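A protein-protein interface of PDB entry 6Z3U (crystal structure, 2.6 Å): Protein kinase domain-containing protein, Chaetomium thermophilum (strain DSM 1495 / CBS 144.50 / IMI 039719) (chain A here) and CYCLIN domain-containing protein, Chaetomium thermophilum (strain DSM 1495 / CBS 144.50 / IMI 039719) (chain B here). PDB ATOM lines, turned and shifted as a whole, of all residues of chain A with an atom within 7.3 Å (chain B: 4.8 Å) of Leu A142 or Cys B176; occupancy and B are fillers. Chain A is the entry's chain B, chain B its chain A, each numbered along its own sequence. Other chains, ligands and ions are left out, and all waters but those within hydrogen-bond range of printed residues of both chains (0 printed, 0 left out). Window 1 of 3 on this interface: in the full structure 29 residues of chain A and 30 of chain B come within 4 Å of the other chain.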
ATOM      1  N   ASN A  85      17.494 -14.575 -15.948  1.00  0.00           N
ATOM      2  CA  ASN A  85      18.557 -15.125 -16.782  1.00  0.00           C
ATOM      3  C   ASN A  85      18.551 -16.646 -16.737  1.00  0.00           C
ATOM      4  O   ASN A  85      18.792 -17.305 -17.756  1.00  0.00           O
ATOM      5  CB  ASN A  85      19.919 -14.589 -16.337  1.00  0.00           C
ATOM      6  CG  ASN A  85      20.385 -13.408 -17.172  1.00  0.00           C
ATOM      7  OD1 ASN A  85      20.268 -13.413 -18.399  1.00  0.00           O
ATOM      8  ND2 ASN A  85      20.930 -12.393 -16.509  1.00  0.00           N
ATOM      9  N   ILE A 124      31.260 -17.428 -24.127  1.00  0.00           N
ATOM     10  CA  ILE A 124      32.382 -16.499 -24.134  1.00  0.00           C
ATOM     11  C   ILE A 124      32.972 -16.466 -22.732  1.00  0.00           C
ATOM     12  O   ILE A 124      32.275 -16.156 -21.760  1.00  0.00           O
ATOM     13  CB  ILE A 124      31.943 -15.100 -24.583  1.00  0.00           C
ATOM     14  CG1 ILE A 124      31.284 -15.163 -25.961  1.00  0.00           C
ATOM     15  CG2 ILE A 124      33.140 -14.155 -24.618  1.00  0.00           C
ATOM     16  CD1 ILE A 124      30.576 -13.883 -26.357  1.00  0.00           C
ATOM     17  N   MET A 134      35.785  -6.527 -19.944  1.00  0.00           N
ATOM     18  CA  MET A 134      35.167  -7.211 -21.073  1.00  0.00           C
ATOM     19  C   MET A 134      35.911  -6.895 -22.367  1.00  0.00           C
ATOM     20  O   MET A 134      36.218  -5.735 -22.655  1.00  0.00           O
ATOM     21  CB  MET A 134      33.697  -6.802 -21.194  1.00  0.00           C
ATOM     22  CG  MET A 134      32.912  -7.639 -22.197  1.00  0.00           C
ATOM     23  SD  MET A 134      31.124  -7.386 -22.168  1.00  0.00           S
ATOM     24  CE  MET A 134      30.763  -7.434 -20.411  1.00  0.00           C
ATOM     25  N   PRO A 136      36.828  -6.251 -26.291  1.00  0.00           N
ATOM     26  CA  PRO A 136      36.082  -5.501 -27.315  1.00  0.00           C
ATOM     27  C   PRO A 136      35.352  -6.390 -28.306  1.00  0.00           C
ATOM     28  O   PRO A 136      34.251  -6.038 -28.749  1.00  0.00           O
ATOM     29  CB  PRO A 136      37.170  -4.656 -27.999  1.00  0.00           C
ATOM     30  CG  PRO A 136      38.465  -5.307 -27.645  1.00  0.00           C
ATOM     31  CD  PRO A 136      38.269  -5.940 -26.309  1.00  0.00           C
ATOM     32  N   ASP A 137      35.927  -7.536 -28.673  1.00  0.00           N
ATOM     33  CA  ASP A 137      35.235  -8.434 -29.589  1.00  0.00           C
ATOM     34  C   ASP A 137      33.921  -8.923 -28.995  1.00  0.00           C
ATOM     35  O   ASP A 137      32.964  -9.181 -29.733  1.00  0.00           O
ATOM     36  CB  ASP A 137      36.135  -9.616 -29.947  1.00  0.00           C
ATOM     37  CG  ASP A 137      36.673 -10.332 -28.724  1.00  0.00           C
ATOM     38  OD1 ASP A 137      36.544  -9.784 -27.612  1.00  0.00           O
ATOM     39  OD2 ASP A 137      37.229 -11.440 -28.874  1.00  0.00           O
ATOM     40  N   ALA A 138      33.854  -9.056 -27.670  1.00  0.00           N
ATOM     41  CA  ALA A 138      32.608  -9.462 -27.028  1.00  0.00           C
ATOM     42  C   ALA A 138      31.588  -8.332 -27.052  1.00  0.00           C
ATOM     43  O   ALA A 138      30.418  -8.544 -27.394  1.00  0.00           O
ATOM     44  CB  ALA A 138      32.882  -9.908 -25.592  1.00  0.00           C
ATOM     45  N   VAL A 139      32.015  -7.118 -26.696  1.00  0.00           N
ATOM     46  CA  VAL A 139      31.100  -5.980 -26.689  1.00  0.00           C
ATOM     47  C   VAL A 139      30.565  -5.713 -28.090  1.00  0.00           C
ATOM     48  O   VAL A 139      29.370  -5.447 -28.275  1.00  0.00           O
ATOM     49  CB  VAL A 139      31.809  -4.740 -26.113  1.00  0.00           C
ATOM     50  CG1 VAL A 139      30.944  -3.512 -26.285  1.00  0.00           C
ATOM     51  CG2 VAL A 139      32.143  -4.957 -24.652  1.00  0.00           C
ATOM     52  N   ARG A 140      31.438  -5.775 -29.097  1.00  0.00           N
ATOM     53  CA  ARG A 140      31.021  -5.470 -30.462  1.00  0.00           C
ATOM     54  C   ARG A 140      30.017  -6.494 -30.974  1.00  0.00           C
ATOM     55  O   ARG A 140      28.987  -6.131 -31.553  1.00  0.00           O
ATOM     56  CB  ARG A 140      32.244  -5.404 -31.379  1.00  0.00           C
ATOM     57  CG  ARG A 140      33.082  -4.147 -31.199  1.00  0.00           C
ATOM     58  CD  ARG A 140      34.470  -4.286 -31.800  1.00  0.00           C
ATOM     59  NE  ARG A 140      35.202  -3.023 -31.747  1.00  0.00           N
ATOM     60  CZ  ARG A 140      36.528  -2.917 -31.729  1.00  0.00           C
ATOM     61  NH1 ARG A 140      37.290  -4.003 -31.742  1.00  0.00           N
ATOM     62  NH2 ARG A 140      37.093  -1.717 -31.687  1.00  0.00           N
ATOM     63  N   GLU A 141      30.306  -7.783 -30.781  1.00  0.00           N
ATOM     64  CA  GLU A 141      29.377  -8.815 -31.227  1.00  0.00           C
ATOM     65  C   GLU A 141      28.015  -8.638 -30.567  1.00  0.00           C
ATOM     66  O   GLU A 141      26.975  -8.713 -31.229  1.00  0.00           O
ATOM     67  CB  GLU A 141      29.947 -10.203 -30.925  1.00  0.00           C
ATOM     68  CG  GLU A 141      31.128 -10.603 -31.805  1.00  0.00           C
ATOM     69  CD  GLU A 141      30.963 -11.982 -32.421  1.00  0.00           C
ATOM     70  OE1 GLU A 141      31.142 -12.982 -31.695  1.00  0.00           O
ATOM     71  OE2 GLU A 141      30.665 -12.061 -33.631  1.00  0.00           O
ATOM     72  N   LEU A 142      28.007  -8.391 -29.259  1.00  0.00           N
ATOM     73  CA  LEU A 142      26.744  -8.248 -28.540  1.00  0.00           C
ATOM     74  C   LEU A 142      25.926  -7.085 -29.087  1.00  0.00           C
ATOM     75  O   LEU A 142      24.696  -7.170 -29.184  1.00  0.00           O
ATOM     76  CB  LEU A 142      27.026  -8.058 -27.050  1.00  0.00           C
ATOM     77  CG  LEU A 142      26.003  -8.605 -26.056  1.00  0.00           C
ATOM     78  CD1 LEU A 142      25.655 -10.046 -26.374  1.00  0.00           C
ATOM     79  CD2 LEU A 142      26.546  -8.491 -24.637  1.00  0.00           C
ATOM     80  N   LYS A 143      26.593  -5.989 -29.448  1.00  0.00           N
ATOM     81  CA  LYS A 143      25.893  -4.804 -29.927  1.00  0.00           C
ATOM     82  C   LYS A 143      25.399  -4.981 -31.358  1.00  0.00           C
ATOM     83  O   LYS A 143      24.211  -4.792 -31.639  1.00  0.00           O
ATOM     84  CB  LYS A 143      26.817  -3.588 -29.829  1.00  0.00           C
ATOM     85  CG  LYS A 143      26.242  -2.295 -30.394  1.00  0.00           C
ATOM     86  CD  LYS A 143      27.281  -1.176 -30.380  1.00  0.00           C
ATOM     87  CE  LYS A 143      26.718   0.121 -30.944  1.00  0.00           C
ATOM     88  NZ  LYS A 143      27.763   1.180 -31.067  1.00  0.00           N
ATOM     89  N   TYR A 144      26.294  -5.348 -32.274  1.00  0.00           N
ATOM     90  CA  TYR A 144      25.974  -5.262 -33.695  1.00  0.00           C
ATOM     91  C   TYR A 144      25.200  -6.471 -34.201  1.00  0.00           C
ATOM     92  O   TYR A 144      24.392  -6.333 -35.126  1.00  0.00           O
ATOM     93  CB  TYR A 144      27.261  -5.068 -34.497  1.00  0.00           C
ATOM     94  CG  TYR A 144      27.937  -3.749 -34.203  1.00  0.00           C
ATOM     95  CD1 TYR A 144      27.230  -2.555 -34.278  1.00  0.00           C
ATOM     96  CD2 TYR A 144      29.272  -3.695 -33.832  1.00  0.00           C
ATOM     97  CE1 TYR A 144      27.836  -1.345 -34.005  1.00  0.00           C
ATOM     98  CE2 TYR A 144      29.889  -2.487 -33.556  1.00  0.00           C
ATOM     99  CZ  TYR A 144      29.165  -1.316 -33.645  1.00  0.00           C
ATOM    100  OH  TYR A 144      29.770  -0.111 -33.370  1.00  0.00           O
ATOM    101  N   LEU A 145      25.417  -7.652 -33.622  1.00  0.00           N
ATOM    102  CA  LEU A 145      24.617  -8.806 -34.018  1.00  0.00           C
ATOM    103  C   LEU A 145      23.144  -8.580 -33.698  1.00  0.00           C
ATOM    104  O   LEU A 145      22.262  -9.012 -34.450  1.00  0.00           O
ATOM    105  CB  LEU A 145      25.135 -10.070 -33.333  1.00  0.00           C
ATOM    106  CG  LEU A 145      26.470 -10.613 -33.851  1.00  0.00           C
ATOM    107  CD1 LEU A 145      26.911 -11.811 -33.029  1.00  0.00           C
ATOM    108  CD2 LEU A 145      26.377 -10.987 -35.321  1.00  0.00           C
ATOM    109  N   ARG A 146      22.857  -7.904 -32.585  1.00  0.00           N
ATOM    110  CA  ARG A 146      21.476  -7.550 -32.278  1.00  0.00           C
ATOM    111  C   ARG A 146      20.970  -6.466 -33.222  1.00  0.00           C
ATOM    112  O   ARG A 146      19.803  -6.480 -33.629  1.00  0.00           O
ATOM    113  CB  ARG A 146      21.370  -7.087 -30.825  1.00  0.00           C
ATOM    114  CG  ARG A 146      20.005  -6.535 -30.436  1.00  0.00           C
ATOM    115  CD  ARG A 146      18.912  -7.572 -30.625  1.00  0.00           C
ATOM    116  NE  ARG A 146      17.585  -7.030 -30.349  1.00  0.00           N
ATOM    117  CZ  ARG A 146      16.873  -6.321 -31.218  1.00  0.00           C
ATOM    118  NH1 ARG A 146      17.357  -6.054 -32.424  1.00  0.00           N
ATOM    119  NH2 ARG A 146      15.673  -5.874 -30.877  1.00  0.00           N
ATOM    120  N   GLU A 147      21.842  -5.525 -33.589  1.00  0.00           N
ATOM    121  CA  GLU A 147      21.435  -4.427 -34.458  1.00  0.00           C
ATOM    122  C   GLU A 147      21.079  -4.929 -35.851  1.00  0.00           C
ATOM    123  O   GLU A 147      20.092  -4.481 -36.446  1.00  0.00           O
ATOM    124  CB  GLU A 147      22.559  -3.390 -34.532  1.00  0.00           C
ATOM    125  CG  GLU A 147      22.129  -1.955 -34.275  1.00  0.00           C
ATOM    126  CD  GLU A 147      23.316  -1.025 -34.080  1.00  0.00           C
ATOM    127  OE1 GLU A 147      23.432  -0.031 -34.828  1.00  0.00           O
ATOM    128  OE2 GLU A 147      24.148  -1.300 -33.189  1.00  0.00           O
ATOM    129  N   LEU A 157      21.484 -13.804 -34.007  1.00  0.00           N
ATOM    130  CA  LEU A 157      21.649 -13.911 -32.557  1.00  0.00           C
ATOM    131  C   LEU A 157      20.274 -14.196 -31.966  1.00  0.00           C
ATOM    132  O   LEU A 157      19.428 -13.303 -31.870  1.00  0.00           O
ATOM    133  CB  LEU A 157      22.265 -12.639 -31.989  1.00  0.00           C
ATOM    134  CG  LEU A 157      22.530 -12.634 -30.483  1.00  0.00           C
ATOM    135  CD1 LEU A 157      23.521 -13.717 -30.102  1.00  0.00           C
ATOM    136  CD2 LEU A 157      23.036 -11.279 -30.039  1.00  0.00           C
ATOM    137  N   SER A 159      19.423 -15.374 -28.829  1.00  0.00           N
ATOM    138  CA  SER A 159      19.214 -14.974 -27.445  1.00  0.00           C
ATOM    139  C   SER A 159      20.567 -14.758 -26.783  1.00  0.00           C
ATOM    140  O   SER A 159      21.609 -15.161 -27.304  1.00  0.00           O
ATOM    141  CB  SER A 159      18.394 -16.025 -26.689  1.00  0.00           C
ATOM    142  OG  SER A 159      18.301 -15.712 -25.312  1.00  0.00           O
ATOM    143  N   VAL A 160      20.531 -14.109 -25.620  1.00  0.00           N
ATOM    144  CA  VAL A 160      21.717 -13.870 -24.803  1.00  0.00           C
ATOM    145  C   VAL A 160      21.334 -14.075 -23.345  1.00  0.00           C
ATOM    146  O   VAL A 160      20.289 -13.593 -22.899  1.00  0.00           O
ATOM    147  CB  VAL A 160      22.287 -12.452 -25.009  1.00  0.00           C
ATOM    148  CG1 VAL A 160      23.514 -12.234 -24.136  1.00  0.00           C
ATOM    149  CG2 VAL A 160      22.629 -12.226 -26.467  1.00  0.00           C
ATOM    150  N   PHE A 161      22.178 -14.789 -22.605  1.00  0.00           N
ATOM    151  CA  PHE A 161      21.959 -14.986 -21.182  1.00  0.00           C
ATOM    152  C   PHE A 161      23.308 -15.126 -20.493  1.00  0.00           C
ATOM    153  O   PHE A 161      24.311 -15.489 -21.113  1.00  0.00           O
ATOM    154  CB  PHE A 161      21.090 -16.221 -20.908  1.00  0.00           C
ATOM    155  CG  PHE A 161      21.699 -17.511 -21.385  1.00  0.00           C
ATOM    156  CD1 PHE A 161      22.599 -18.205 -20.589  1.00  0.00           C
ATOM    157  CD2 PHE A 161      21.369 -18.035 -22.623  1.00  0.00           C
ATOM    158  CE1 PHE A 161      23.162 -19.390 -21.024  1.00  0.00           C
ATOM    159  CE2 PHE A 161      21.927 -19.223 -23.062  1.00  0.00           C
ATOM    160  CZ  PHE A 161      22.824 -19.900 -22.261  1.00  0.00           C
ATOM    161  N   LEU A 168      29.493 -15.080 -20.351  1.00  0.00           N
ATOM    162  CA  LEU A 168      28.551 -14.608 -21.355  1.00  0.00           C
ATOM    163  C   LEU A 168      28.265 -15.719 -22.357  1.00  0.00           C
ATOM    164  O   LEU A 168      29.190 -16.391 -22.828  1.00  0.00           O
ATOM    165  CB  LEU A 168      29.103 -13.377 -22.070  1.00  0.00           C
ATOM    166  CG  LEU A 168      28.154 -12.676 -23.039  1.00  0.00           C
ATOM    167  CD1 LEU A 168      26.926 -12.160 -22.308  1.00  0.00           C
ATOM    168  CD2 LEU A 168      28.870 -11.545 -23.757  1.00  0.00           C
ATOM    169  N   ASN A 169      26.991 -15.904 -22.683  1.00  0.00           N
ATOM    170  CA  ASN A 169      26.563 -16.955 -23.595  1.00  0.00           C
ATOM    171  C   ASN A 169      25.754 -16.348 -24.729  1.00  0.00           C
ATOM    172  O   ASN A 169      24.850 -15.542 -24.489  1.00  0.00           O
ATOM    173  CB  ASN A 169      25.731 -18.019 -22.873  1.00  0.00           C
ATOM    174  CG  ASN A 169      26.494 -18.693 -21.753  1.00  0.00           C
ATOM    175  OD1 ASN A 169      26.493 -18.220 -20.618  1.00  0.00           O
ATOM    176  ND2 ASN A 169      27.154 -19.803 -22.067  1.00  0.00           N
ATOM    177  N   LEU A 170      26.085 -16.735 -25.958  1.00  0.00           N
ATOM    178  CA  LEU A 170      25.380 -16.283 -27.148  1.00  0.00           C
ATOM    179  C   LEU A 170      24.693 -17.476 -27.798  1.00  0.00           C
ATOM    180  O   LEU A 170      25.361 -18.425 -28.223  1.00  0.00           O
ATOM    181  CB  LEU A 170      26.339 -15.633 -28.143  1.00  0.00           C
ATOM    182  CG  LEU A 170      27.194 -14.478 -27.629  1.00  0.00           C
ATOM    183  CD1 LEU A 170      28.014 -13.900 -28.773  1.00  0.00           C
ATOM    184  CD2 LEU A 170      26.334 -13.411 -26.979  1.00  0.00           C
ATOM    185  N   PHE A 239      31.912 -10.508 -35.986  1.00  0.00           N
ATOM    186  CA  PHE A 239      31.761  -9.061 -35.889  1.00  0.00           C
ATOM    187  C   PHE A 239      32.639  -8.459 -34.799  1.00  0.00           C
ATOM    188  O   PHE A 239      32.381  -7.341 -34.345  1.00  0.00           O
ATOM    189  CB  PHE A 239      30.292  -8.703 -35.645  1.00  0.00           C
ATOM    190  CG  PHE A 239      29.474  -8.610 -36.903  1.00  0.00           C
ATOM    191  CD1 PHE A 239      28.979  -9.749 -37.515  1.00  0.00           C
ATOM    192  CD2 PHE A 239      29.182  -7.377 -37.460  1.00  0.00           C
ATOM    193  CE1 PHE A 239      28.226  -9.658 -38.671  1.00  0.00           C
ATOM    194  CE2 PHE A 239      28.428  -7.282 -38.612  1.00  0.00           C
ATOM    195  CZ  PHE A 239      27.950  -8.423 -39.217  1.00  0.00           C
ATOM    196  N   PHE B 142      31.696   1.472 -19.278  1.00  0.00           N
ATOM    197  CA  PHE B 142      31.029   0.605 -20.243  1.00  0.00           C
ATOM    198  C   PHE B 142      30.399   1.412 -21.373  1.00  0.00           C
ATOM    199  O   PHE B 142      30.273   0.910 -22.496  1.00  0.00           O
ATOM    200  CB  PHE B 142      29.977  -0.245 -19.531  1.00  0.00           C
ATOM    201  CG  PHE B 142      29.625  -1.510 -20.259  1.00  0.00           C
ATOM    202  CD1 PHE B 142      30.582  -2.491 -20.467  1.00  0.00           C
ATOM    203  CD2 PHE B 142      28.338  -1.728 -20.716  1.00  0.00           C
ATOM    204  CE1 PHE B 142      30.263  -3.659 -21.132  1.00  0.00           C
ATOM    205  CE2 PHE B 142      28.011  -2.896 -21.380  1.00  0.00           C
ATOM    206  CZ  PHE B 142      28.974  -3.863 -21.587  1.00  0.00           C
ATOM    207  N   GLU B 172      31.299  -4.166 -14.062  1.00  0.00           N
ATOM    208  CA  GLU B 172      31.117  -4.121 -15.510  1.00  0.00           C
ATOM    209  C   GLU B 172      30.123  -5.181 -15.973  1.00  0.00           C
ATOM    210  O   GLU B 172      29.110  -4.867 -16.607  1.00  0.00           O
ATOM    211  CB  GLU B 172      32.461  -4.296 -16.220  1.00  0.00           C
ATOM    212  CG  GLU B 172      32.393  -4.003 -17.716  1.00  0.00           C
ATOM    213  CD  GLU B 172      33.682  -4.328 -18.451  1.00  0.00           C
ATOM    214  OE1 GLU B 172      33.997  -3.626 -19.436  1.00  0.00           O
ATOM    215  OE2 GLU B 172      34.377  -5.286 -18.052  1.00  0.00           O
ATOM    216  N   PHE B 173      30.400  -6.451 -15.667  1.00  0.00           N
ATOM    217  CA  PHE B 173      29.503  -7.516 -16.104  1.00  0.00           C
ATOM    218  C   PHE B 173      28.145  -7.403 -15.423  1.00  0.00           C
ATOM    219  O   PHE B 173      27.112  -7.716 -16.026  1.00  0.00           O
ATOM    220  CB  PHE B 173      30.125  -8.883 -15.827  1.00  0.00           C
ATOM    221  CG  PHE B 173      29.412 -10.018 -16.506  1.00  0.00           C
ATOM    222  CD1 PHE B 173      29.307 -10.058 -17.887  1.00  0.00           C
ATOM    223  CD2 PHE B 173      28.844 -11.041 -15.765  1.00  0.00           C
ATOM    224  CE1 PHE B 173      28.652 -11.098 -18.518  1.00  0.00           C
ATOM    225  CE2 PHE B 173      28.187 -12.084 -16.390  1.00  0.00           C
ATOM    226  CZ  PHE B 173      28.091 -12.113 -17.769  1.00  0.00           C
ATOM    227  N   LEU B 174      28.130  -6.970 -14.164  1.00  0.00           N
ATOM    228  CA  LEU B 174      26.863  -6.748 -13.479  1.00  0.00           C
ATOM    229  C   LEU B 174      26.006  -5.742 -14.241  1.00  0.00           C
ATOM    230  O   LEU B 174      24.810  -5.967 -14.464  1.00  0.00           O
ATOM    231  CB  LEU B 174      27.127  -6.272 -12.051  1.00  0.00           C
ATOM    232  CG  LEU B 174      25.901  -6.130 -11.149  1.00  0.00           C
ATOM    233  CD1 LEU B 174      25.268  -7.492 -10.877  1.00  0.00           C
ATOM    234  CD2 LEU B 174      26.275  -5.433  -9.849  1.00  0.00           C
ATOM    235  N   LEU B 175      26.609  -4.629 -14.662  1.00  0.00           N
ATOM    236  CA  LEU B 175      25.874  -3.646 -15.451  1.00  0.00           C
ATOM    237  C   LEU B 175      25.359  -4.259 -16.747  1.00  0.00           C
ATOM    238  O   LEU B 175      24.224  -3.995 -17.162  1.00  0.00           O
ATOM    239  CB  LEU B 175      26.769  -2.442 -15.747  1.00  0.00           C
ATOM    240  CG  LEU B 175      26.201  -1.377 -16.686  1.00  0.00           C
ATOM    241  CD1 LEU B 175      25.038  -0.645 -16.032  1.00  0.00           C
ATOM    242  CD2 LEU B 175      27.287  -0.399 -17.110  1.00  0.00           C
ATOM    243  N   CYS B 176      26.178  -5.088 -17.397  1.00  0.00           N
ATOM    244  CA  CYS B 176      25.769  -5.677 -18.666  1.00  0.00           C
ATOM    245  C   CYS B 176      24.479  -6.471 -18.503  1.00  0.00           C
ATOM    246  O   CYS B 176      23.568  -6.368 -19.332  1.00  0.00           O
ATOM    247  CB  CYS B 176      26.889  -6.560 -19.213  1.00  0.00           C
ATOM    248  SG  CYS B 176      26.741  -6.958 -20.968  1.00  0.00           S
ATOM    249  N   GLN B 177      24.380  -7.262 -17.432  1.00  0.00           N
ATOM    250  CA  GLN B 177      23.141  -7.985 -17.168  1.00  0.00           C
ATOM    251  C   GLN B 177      21.996  -7.026 -16.866  1.00  0.00           C
ATOM    252  O   GLN B 177      20.869  -7.230 -17.331  1.00  0.00           O
ATOM    253  CB  GLN B 177      23.332  -8.956 -16.002  1.00  0.00           C
ATOM    254  CG  GLN B 177      24.474  -9.949 -16.160  1.00  0.00           C
ATOM    255  CD  GLN B 177      24.693 -10.786 -14.907  1.00  0.00           C
ATOM    256  OE1 GLN B 177      24.089 -11.845 -14.753  1.00  0.00           O
ATOM    257  NE2 GLN B 177      25.646 -10.378 -14.074  1.00  0.00           N
ATOM    258  N   GLY B 178      22.267  -5.972 -16.094  1.00  0.00           N
ATOM    259  CA  GLY B 178      21.202  -5.067 -15.703  1.00  0.00           C
ATOM    260  C   GLY B 178      20.512  -4.420 -16.888  1.00  0.00           C
ATOM    261  O   GLY B 178      19.284  -4.297 -16.910  1.00  0.00           O
ATOM    262  N   ILE B 179      21.286  -4.013 -17.894  1.00  0.00           N
ATOM    263  CA  ILE B 179      20.735  -3.369 -19.082  1.00  0.00           C
ATOM    264  C   ILE B 179      20.259  -4.435 -20.062  1.00  0.00           C
ATOM    265  O   ILE B 179      19.887  -4.128 -21.200  1.00  0.00           O
ATOM    266  CB  ILE B 179      21.760  -2.428 -19.740  1.00  0.00           C
ATOM    267  CG1 ILE B 179      22.993  -3.202 -20.216  1.00  0.00           C
ATOM    268  CG2 ILE B 179      22.168  -1.332 -18.766  1.00  0.00           C
ATOM    269  CD1 ILE B 179      23.967  -2.358 -21.014  1.00  0.00           C
ATOM    270  N   ARG B 180      20.280  -5.694 -19.627  1.00  0.00           N
ATOM    271  CA  ARG B 180      19.727  -6.800 -20.407  1.00  0.00           C
ATOM    272  C   ARG B 180      20.466  -6.973 -21.732  1.00  0.00           C
ATOM    273  O   ARG B 180      19.877  -7.333 -22.753  1.00  0.00           O
ATOM    274  CB  ARG B 180      18.228  -6.599 -20.640  1.00  0.00           C
ATOM    275  CG  ARG B 180      17.397  -6.669 -19.367  1.00  0.00           C
ATOM    276  CD  ARG B 180      15.924  -6.861 -19.681  1.00  0.00           C
ATOM    277  NE  ARG B 180      15.669  -8.170 -20.276  1.00  0.00           N
ATOM    278  CZ  ARG B 180      14.503  -8.546 -20.791  1.00  0.00           C
ATOM    279  NH1 ARG B 180      14.367  -9.757 -21.312  1.00  0.00           N
ATOM    280  NH2 ARG B 180      13.474  -7.708 -20.792  1.00  0.00           N
ATOM    281  N   PHE B 181      21.774  -6.726 -21.715  1.00  0.00           N
ATOM    282  CA  PHE B 181      22.643  -6.989 -22.858  1.00  0.00           C
ATOM    283  C   PHE B 181      22.277  -6.150 -24.078  1.00  0.00           C
ATOM    284  O   PHE B 181      22.669  -6.481 -25.201  1.00  0.00           O
ATOM    285  CB  PHE B 181      22.618  -8.477 -23.225  1.00  0.00           C
ATOM    286  CG  PHE B 181      22.907  -9.391 -22.069  1.00  0.00           C
ATOM    287  CD1 PHE B 181      24.212  -9.694 -21.719  1.00  0.00           C
ATOM    288  CD2 PHE B 181      21.875  -9.944 -21.328  1.00  0.00           C
ATOM    289  CE1 PHE B 181      24.483 -10.533 -20.657  1.00  0.00           C
ATOM    290  CE2 PHE B 181      22.141 -10.785 -20.264  1.00  0.00           C
ATOM    291  CZ  PHE B 181      23.446 -11.080 -19.928  1.00  0.00           C
ATOM    292  N   LEU B 183      23.090  -3.070 -25.940  1.00  0.00           N
ATOM    293  CA  LEU B 183      24.168  -2.094 -26.025  1.00  0.00           C
ATOM    294  C   LEU B 183      23.929  -1.015 -27.074  1.00  0.00           C
ATOM    295  O   LEU B 183      24.662  -0.018 -27.087  1.00  0.00           O
ATOM    296  CB  LEU B 183      25.493  -2.803 -26.327  1.00  0.00           C
ATOM    297  CG  LEU B 183      26.243  -3.375 -25.121  1.00  0.00           C
ATOM    298  CD1 LEU B 183      25.311  -4.131 -24.195  1.00  0.00           C
ATOM    299  CD2 LEU B 183      27.373  -4.273 -25.586  1.00  0.00           C
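Of the 23 printed residues of chain A, 7 touch a printed residue of chain B.
Printed residues of chain A that touch a printed residue of chain B: Asn A85, Met A134, Val A139, Leu A142, Lys A143, Val A160 and Leu A168.
Hydrophobic or aromatic side chains of chain A that line the printed part of chain B: Met A134, Val A139, Leu A142, Val A160 and Leu A168.
Of the 12 printed residues of chain B, 7 touch a printed residue of chain A.
Hydrophobic or aromatic side chains of chain B that line the printed part of chain A: Phe B142, Phe B173, Phe B181 and Leu B183.
Among the printed residues, 11 pairs touch across the chains.
The side-chain carboxylate of Glu B172 sits at hydrogen-bond distance from the backbone NH of Met A134, at 2.7 Å.
Among the printed residues, merely in contact across the chains: Leu A168 with Phe B181 (3.4 Å), Val A139 with Leu B183 (3.5 Å), Val A160 with Phe B181 (3.6 Å), Asn A85 with Gln B177 (3.7 Å), Asn A85 with Phe B181 (3.7 Å), Lys A143 with Leu B183 (3.8 Å), Met A134 with Phe B142 (3.9 Å), Met A134 with Phe B173 (3.9 Å), Leu A142 with Phe B181 (3.9 Å) and Leu A142 with Cys B176 (3.98 Å).
O of Cys B176 is in hydrogen-bond range of N of Phe B181.
The backbone NH (N) of Ile A124 is in hydrogen-bond range of the backbone carbonyl oxygen (O) of Leu A168, at 2.7 Å.
NZ of Lys A143 sits at hydrogen-bond distance from OH of Tyr A144.
Printed residues of chain B within 4 Å of Leu A142: Cys B176 (3.98 Å) and Phe B181 (3.9 Å).
Of the printed residues of chain A, Glu B172 touches Met A134 (2.7 Å).
Of the printed residues of chain A, Phe B173 touches Met A134.
Ala A138 touches none of the printed residues of chain B.
Arg B180 touches none of the printed residues of chain A.
The nearest printed residue of chain B that does not touch Leu A142 is Leu B183 (4.1 Å).
The nearest printed residue of chain B that does not touch Val A160 is Arg B180 (6.1 Å).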
